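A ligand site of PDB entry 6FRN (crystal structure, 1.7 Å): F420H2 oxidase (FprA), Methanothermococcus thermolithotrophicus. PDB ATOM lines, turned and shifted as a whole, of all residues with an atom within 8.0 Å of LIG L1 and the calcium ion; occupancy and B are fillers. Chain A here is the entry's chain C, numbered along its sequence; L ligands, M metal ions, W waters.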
ATOM      1  N   PHE A  41     -21.363 -22.960   6.757  1.00  0.00           N
ATOM      2  CA  PHE A  41     -20.025 -23.200   7.255  1.00  0.00           C
ATOM      3  C   PHE A  41     -19.408 -24.330   6.524  1.00  0.00           C
ATOM      4  O   PHE A  41     -19.716 -25.486   6.822  1.00  0.00           O
ATOM      5  CB  PHE A  41     -20.063 -23.605   8.741  1.00  0.00           C
ATOM      6  CG  PHE A  41     -20.434 -22.478   9.674  1.00  0.00           C
ATOM      7  CD1 PHE A  41     -21.754 -22.200   9.958  1.00  0.00           C
ATOM      8  CD2 PHE A  41     -19.458 -21.717  10.303  1.00  0.00           C
ATOM      9  CE1 PHE A  41     -22.097 -21.170  10.820  1.00  0.00           C
ATOM     10  CE2 PHE A  41     -19.796 -20.645  11.111  1.00  0.00           C
ATOM     11  CZ  PHE A  41     -21.127 -20.387  11.378  1.00  0.00           C
ATOM     12  N   GLY A  42     -18.497 -24.060   5.615  1.00  0.00           N
ATOM     13  CA  GLY A  42     -17.702 -25.116   5.023  1.00  0.00           C
ATOM     14  C   GLY A  42     -16.573 -25.399   5.999  1.00  0.00           C
ATOM     15  O   GLY A  42     -16.542 -24.828   7.107  1.00  0.00           O
ATOM     16  N   ASP A  43     -15.652 -26.275   5.637  1.00  0.00           N
ATOM     17  CA  ASP A  43     -14.496 -26.593   6.465  1.00  0.00           C
ATOM     18  C   ASP A  43     -13.587 -25.392   6.637  1.00  0.00           C
ATOM     19  O   ASP A  43     -12.970 -25.241   7.663  1.00  0.00           O
ATOM     20  CB  ASP A  43     -13.663 -27.748   5.896  1.00  0.00           C
ATOM     21  CG  ASP A  43     -14.372 -29.094   5.887  1.00  0.00           C
ATOM     22  OD1 ASP A  43     -15.309 -29.283   6.688  1.00  0.00           O
ATOM     23  OD2 ASP A  43     -13.966 -29.963   5.088  1.00  0.00           O
ATOM     24  N   ASP A  44     -13.420 -24.612   5.566  1.00  0.00           N
ATOM     25  CA  ASP A  44     -12.512 -23.494   5.500  1.00  0.00           C
ATOM     26  C   ASP A  44     -13.183 -22.123   5.462  1.00  0.00           C
ATOM     27  O   ASP A  44     -12.657 -21.182   6.033  1.00  0.00           O
ATOM     28  CB  ASP A  44     -11.644 -23.625   4.237  1.00  0.00           C
ATOM     29  CG  ASP A  44     -11.229 -25.058   3.904  1.00  0.00           C
ATOM     30  OD1 ASP A  44     -11.093 -25.870   4.842  1.00  0.00           O
ATOM     31  OD2 ASP A  44     -11.074 -25.366   2.701  1.00  0.00           O
ATOM     32  N   LYS A  45     -14.312 -21.968   4.753  1.00  0.00           N
ATOM     33  CA  LYS A  45     -14.910 -20.661   4.623  1.00  0.00           C
ATOM     34  C   LYS A  45     -16.364 -20.664   5.050  1.00  0.00           C
ATOM     35  O   LYS A  45     -17.014 -21.695   4.967  1.00  0.00           O
ATOM     36  CB  LYS A  45     -14.785 -20.192   3.157  1.00  0.00           C
ATOM     37  CG  LYS A  45     -13.343 -20.039   2.712  1.00  0.00           C
ATOM     38  CD  LYS A  45     -13.214 -19.680   1.257  1.00  0.00           C
ATOM     39  CE  LYS A  45     -11.749 -19.588   0.884  1.00  0.00           C
ATOM     40  NZ  LYS A  45     -11.564 -19.397  -0.562  1.00  0.00           N
ATOM     41  N   VAL A  46     -16.849 -19.519   5.528  1.00  0.00           N
ATOM     42  CA  VAL A  46     -18.255 -19.328   5.904  1.00  0.00           C
ATOM     43  C   VAL A  46     -18.863 -18.388   4.925  1.00  0.00           C
ATOM     44  O   VAL A  46     -18.298 -17.323   4.707  1.00  0.00           O
ATOM     45  CB  VAL A  46     -18.444 -18.748   7.334  1.00  0.00           C
ATOM     46  CG1 VAL A  46     -19.902 -18.831   7.766  1.00  0.00           C
ATOM     47  CG2 VAL A  46     -17.575 -19.465   8.312  1.00  0.00           C
ATOM     48  N   CYS A  68     -21.753 -19.151  15.022  1.00  0.00           N
ATOM     49  CA  CYS A  68     -20.280 -19.322  15.111  1.00  0.00           C
ATOM     50  C   CYS A  68     -19.915 -20.032  16.403  1.00  0.00           C
ATOM     51  O   CYS A  68     -19.183 -21.038  16.389  1.00  0.00           O
ATOM     52  CB  CYS A  68     -19.569 -17.961  14.993  1.00  0.00           C
ATOM     53  SG  CYS A  68     -19.629 -17.235  13.327  1.00  0.00           S
ATOM     54  N   GLU A  71     -20.824 -23.712  16.379  1.00  0.00           N
ATOM     55  CA  GLU A  71     -19.893 -24.432  15.502  1.00  0.00           C
ATOM     56  C   GLU A  71     -18.465 -24.489  16.068  1.00  0.00           C
ATOM     57  O   GLU A  71     -17.649 -25.225  15.533  1.00  0.00           O
ATOM     58  CB  GLU A  71     -19.863 -23.790  14.109  1.00  0.00           C
ATOM     59  CG  GLU A  71     -21.113 -24.038  13.321  1.00  0.00           C
ATOM     60  CD  GLU A  71     -21.242 -25.485  12.890  1.00  0.00           C
ATOM     61  OE1 GLU A  71     -20.230 -26.073  12.442  1.00  0.00           O
ATOM     62  OE2 GLU A  71     -22.334 -26.044  13.080  1.00  0.00           O
ATOM     63  N   GLY A  72     -18.163 -23.733  17.117  1.00  0.00           N
ATOM     64  CA  GLY A  72     -16.818 -23.653  17.670  1.00  0.00           C
ATOM     65  C   GLY A  72     -15.900 -22.910  16.714  1.00  0.00           C
ATOM     66  O   GLY A  72     -14.726 -23.231  16.632  1.00  0.00           O
ATOM     67  N   ARG A  73     -16.430 -21.864  16.027  1.00  0.00           N
ATOM     68  CA  ARG A  73     -15.715 -21.100  15.040  1.00  0.00           C
ATOM     69  C   ARG A  73     -15.578 -19.663  15.464  1.00  0.00           C
ATOM     70  O   ARG A  73     -16.397 -19.144  16.205  1.00  0.00           O
ATOM     71  CB  ARG A  73     -16.453 -21.137  13.689  1.00  0.00           C
ATOM     72  CG  ARG A  73     -16.550 -22.506  13.044  1.00  0.00           C
ATOM     73  CD  ARG A  73     -15.294 -23.008  12.444  1.00  0.00           C
ATOM     74  NE  ARG A  73     -15.607 -24.277  11.825  1.00  0.00           N
ATOM     75  CZ  ARG A  73     -15.941 -24.468  10.556  1.00  0.00           C
ATOM     76  NH1 ARG A  73     -15.930 -23.460   9.680  1.00  0.00           N
ATOM     77  NH2 ARG A  73     -16.251 -25.682  10.125  1.00  0.00           N
ATOM     78  N   GLU A  74     -14.574 -18.999  14.973  1.00  0.00           N
ATOM     79  CA  GLU A  74     -14.413 -17.566  15.215  1.00  0.00           C
ATOM     80  C   GLU A  74     -15.547 -16.791  14.556  1.00  0.00           C
ATOM     81  O   GLU A  74     -16.181 -17.276  13.609  1.00  0.00           O
ATOM     82  CB  GLU A  74     -13.054 -17.074  14.693  1.00  0.00           C
ATOM     83  CG  GLU A  74     -12.935 -17.105  13.173  1.00  0.00           C
ATOM     84  CD  GLU A  74     -11.594 -16.606  12.727  1.00  0.00           C
ATOM     85  OE1 GLU A  74     -11.348 -15.385  12.830  1.00  0.00           O
ATOM     86  OE2 GLU A  74     -10.762 -17.435  12.319  1.00  0.00           O
ATOM     87  N   PHE A  75     -15.764 -15.563  15.027  1.00  0.00           N
ATOM     88  CA  PHE A  75     -16.778 -14.685  14.451  1.00  0.00           C
ATOM     89  C   PHE A  75     -16.176 -14.088  13.172  1.00  0.00           C
ATOM     90  O   PHE A  75     -15.440 -13.111  13.214  1.00  0.00           O
ATOM     91  CB  PHE A  75     -17.177 -13.591  15.444  1.00  0.00           C
ATOM     92  CG  PHE A  75     -18.059 -12.496  14.877  1.00  0.00           C
ATOM     93  CD1 PHE A  75     -19.250 -12.797  14.258  1.00  0.00           C
ATOM     94  CD2 PHE A  75     -17.721 -11.152  15.046  1.00  0.00           C
ATOM     95  CE1 PHE A  75     -20.081 -11.771  13.753  1.00  0.00           C
ATOM     96  CE2 PHE A  75     -18.536 -10.146  14.542  1.00  0.00           C
ATOM     97  CZ  PHE A  75     -19.717 -10.455  13.903  1.00  0.00           C
ATOM     98  N   LYS A  76     -16.441 -14.749  12.031  1.00  0.00           N
ATOM     99  CA  LYS A  76     -15.913 -14.345  10.736  1.00  0.00           C
ATOM    100  C   LYS A  76     -16.807 -14.826   9.585  1.00  0.00           C
ATOM    101  O   LYS A  76     -17.216 -15.988   9.570  1.00  0.00           O
ATOM    102  CB  LYS A  76     -14.516 -14.923  10.559  1.00  0.00           C
ATOM    103  CG  LYS A  76     -13.829 -14.551   9.254  1.00  0.00           C
ATOM    104  CD  LYS A  76     -12.439 -15.163   9.210  1.00  0.00           C
ATOM    105  CE  LYS A  76     -11.723 -14.861   7.921  1.00  0.00           C
ATOM    106  NZ  LYS A  76     -10.788 -13.757   8.037  1.00  0.00           N
ATOM    107  N   ASP A  78     -16.544 -15.105   5.443  1.00  0.00           N
ATOM    108  CA  ASP A  78     -15.580 -15.096   4.332  1.00  0.00           C
ATOM    109  C   ASP A  78     -16.147 -14.695   2.997  1.00  0.00           C
ATOM    110  O   ASP A  78     -15.385 -14.262   2.140  1.00  0.00           O
ATOM    111  CB  ASP A  78     -15.010 -16.476   4.157  1.00  0.00           C
ATOM    112  CG  ASP A  78     -14.253 -16.934   5.358  1.00  0.00           C
ATOM    113  OD1 ASP A  78     -13.199 -16.369   5.626  1.00  0.00           O
ATOM    114  OD2 ASP A  78     -14.734 -17.869   6.041  1.00  0.00           O
ATOM    115  N   LEU A 138     -16.357 -24.012  -0.408  1.00  0.00           N
ATOM    116  CA  LEU A 138     -16.136 -23.530   0.971  1.00  0.00           C
ATOM    117  C   LEU A 138     -15.366 -24.539   1.825  1.00  0.00           C
ATOM    118  O   LEU A 138     -15.080 -24.248   2.992  1.00  0.00           O
ATOM    119  CB  LEU A 138     -17.490 -23.265   1.634  1.00  0.00           C
ATOM    120  CG  LEU A 138     -18.390 -22.297   0.919  1.00  0.00           C
ATOM    121  CD1 LEU A 138     -19.751 -22.302   1.565  1.00  0.00           C
ATOM    122  CD2 LEU A 138     -17.794 -20.866   0.938  1.00  0.00           C
HETATM  123  C1  LIG L   1     -11.193 -22.732  12.257  1.00  0.00           C
HETATM  124  C2  LIG L   1      -7.143 -16.451  11.753  1.00  0.00           C
HETATM  125  C3  LIG L   1      -8.748 -21.834  11.638  1.00  0.00           C
HETATM  126  C4  LIG L   1      -5.667 -18.764  12.516  1.00  0.00           C
HETATM  127  C5  LIG L   1      -5.548 -20.304  12.628  1.00  0.00           C
HETATM  128  C6  LIG L   1      -6.204 -18.336  14.810  1.00  0.00           C
HETATM  129  C7  LIG L   1      -6.430 -19.754  15.337  1.00  0.00           C
HETATM  130  C8  LIG L   1      -7.545 -21.776  14.789  1.00  0.00           C
HETATM  131  C9  LIG L   1      -6.781 -22.143  13.533  1.00  0.00           C
HETATM  132  C10 LIG L   1      -6.818 -15.321  10.999  1.00  0.00           C
HETATM  133  C11 LIG L   1      -7.310 -15.189   9.736  1.00  0.00           C
HETATM  134  C12 LIG L   1      -8.119 -16.164   9.206  1.00  0.00           C
HETATM  135  C13 LIG L   1      -8.419 -17.283   9.992  1.00  0.00           C
HETATM  136  C14 LIG L   1      -9.297 -18.446   9.568  1.00  0.00           C
HETATM  137  C15 LIG L   1      -9.156 -23.051  11.129  1.00  0.00           C
HETATM  138  C16 LIG L   1     -10.403 -23.502  11.439  1.00  0.00           C
HETATM  139  C17 LIG L   1     -10.713 -21.522  12.760  1.00  0.00           C
HETATM  140  C18 LIG L   1     -11.604 -20.670  13.668  1.00  0.00           C
HETATM  141  C19 LIG L   1      -7.360 -21.277  11.357  1.00  0.00           C
HETATM  142  C20 LIG L   1      -6.638 -16.708  13.185  1.00  0.00           C
HETATM  143  N1  LIG L   1      -6.671 -18.169  13.450  1.00  0.00           N
HETATM  144  N2  LIG L   1      -7.652 -20.329  14.783  1.00  0.00           N
HETATM  145  N3  LIG L   1      -6.879 -20.961  12.663  1.00  0.00           N
HETATM  146  N4  LIG L   1      -7.925 -17.395  11.228  1.00  0.00           N
HETATM  147  N5  LIG L   1      -9.499 -21.082  12.438  1.00  0.00           N
HETATM  148  O1  LIG L   1     -12.782 -21.035  13.911  1.00  0.00           O
HETATM  149  O2  LIG L   1     -11.166 -19.611  14.167  1.00  0.00           O
HETATM  150  O3  LIG L   1      -9.663 -18.620   8.374  1.00  0.00           O
HETATM  151  O4  LIG L   1      -9.655 -19.212  10.508  1.00  0.00           O
HETATM  152 TB1  LIG L   1      -9.057 -19.120  12.863  1.00  0.00          TB
HETATM  153  C1  LG2 L   2     -12.868 -19.329  10.172  1.00  0.00           C
HETATM  154  O1  LG2 L   2     -11.984 -20.315   9.751  1.00  0.00           O
HETATM  155  C2  LG2 L   2     -13.877 -19.195   9.043  1.00  0.00           C
HETATM  156  O2  LG2 L   2     -13.163 -18.936   7.845  1.00  0.00           O
HETATM  157  C3  LG2 L   2     -14.633 -20.521   8.943  1.00  0.00           C
HETATM  158  O3  LG2 L   2     -15.617 -20.629   9.969  1.00  0.00           O
HETATM  159  C1  LG3 L   3     -10.199 -15.417  16.263  1.00  0.00           C
HETATM  160  C2  LG3 L   3     -11.153 -21.362  17.267  1.00  0.00           C
HETATM  161  C3  LG3 L   3     -10.661 -16.006  18.887  1.00  0.00           C
HETATM  162  C4  LG3 L   3     -13.058 -18.506  18.865  1.00  0.00           C
HETATM  163  C5  LG3 L   3     -12.823 -17.813  20.231  1.00  0.00           C
HETATM  164  C6  LG3 L   3     -12.823 -20.741  19.651  1.00  0.00           C
HETATM  165  C7  LG3 L   3     -11.707 -21.450  20.425  1.00  0.00           C
HETATM  166  C8  LG3 L   3     -11.499 -19.662  22.005  1.00  0.00           C
HETATM  167  C9  LG3 L   3     -11.106 -18.187  21.878  1.00  0.00           C
HETATM  168  C10 LG3 L   3     -11.430 -22.485  16.494  1.00  0.00           C
HETATM  169  C11 LG3 L   3     -10.508 -23.469  16.384  1.00  0.00           C
HETATM  170  C12 LG3 L   3      -9.311 -23.359  17.026  1.00  0.00           C
HETATM  171  C13 LG3 L   3      -9.048 -22.226  17.798  1.00  0.00           C
HETATM  172  C14 LG3 L   3      -7.699 -22.101  18.524  1.00  0.00           C
HETATM  173  C15 LG3 L   3     -10.811 -14.708  18.436  1.00  0.00           C
HETATM  174  C16 LG3 L   3     -10.569 -14.418  17.121  1.00  0.00           C
HETATM  175  C17 LG3 L   3     -10.052 -16.726  16.743  1.00  0.00           C
HETATM  176  C18 LG3 L   3      -9.636 -17.840  15.787  1.00  0.00           C
HETATM  177  C19 LG3 L   3     -10.932 -16.323  20.375  1.00  0.00           C
HETATM  178  C20 LG3 L   3     -12.212 -20.226  17.393  1.00  0.00           C
HETATM  179  N1  LG3 L   3     -12.243 -19.736  18.790  1.00  0.00           N
HETATM  180  N2  LG3 L   3     -10.799 -20.451  21.004  1.00  0.00           N
HETATM  181  N3  LG3 L   3     -11.372 -17.720  20.512  1.00  0.00           N
HETATM  182  N4  LG3 L   3      -9.970 -21.243  17.908  1.00  0.00           N
HETATM  183  N5  LG3 L   3     -10.287 -16.996  18.051  1.00  0.00           N
HETATM  184  O1  LG3 L   3      -9.578 -19.031  16.195  1.00  0.00           O
HETATM  185  O2  LG3 L   3      -9.336 -17.581  14.593  1.00  0.00           O
HETATM  186  O3  LG3 L   3      -6.855 -23.029  18.449  1.00  0.00           O
HETATM  187  O4  LG3 L   3      -7.446 -21.066  19.192  1.00  0.00           O
HETATM  188 TB1  LG3 L   3      -9.741 -19.207  18.900  1.00  0.00          TB
HETATM  189 CA    CA M   1     -11.097 -20.060   7.270  1.00  0.00          CA
HETATM  190  O   HOH W   1      -8.861 -20.846   7.749  1.00  0.00           O
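Arg 73 touches LIG L1 (CA to O1, 3.1 Å). NZ of Lys 76 touches C12 of LIG L1, at 3.8 Å. The nearest printed residue that does not touch LIG L1 is Gly 72 (4.001 Å).
N of Glu 74 is in hydrogen-bond range of O1 of LIG L1 (2.9 Å). The side-chain carboxylate of Glu 74 binds a terbium atom (TB1) of LIG L1, at 2.5 Å.
The calcium ion is bound by O of Asp 44 (2.3 Å), O3 of LIG L1 (2.3 Å), water W1 (2.4 Å), O2 of LG2 L2 (2.4 Å) and O1 of LG2 L2 (2.6 Å).
The backbone NH of Asp 44 sits at hydrogen-bond distance from the backbone carbonyl oxygen of Leu 138. O of Glu 74 sits at hydrogen-bond distance from SG of Cys 68, at 3.5 Å. The backbone NH (N) of Arg 73 lies within hydrogen-bond range of the backbone carbonyl oxygen (O) of Cys 68 (2.9 Å). NH1 of Arg 73 lies within hydrogen-bond range of O of Gly 42 (3.0 Å).
TB1 of LIG L1 is bound by O2 of LG3 L3 (2.3 Å).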
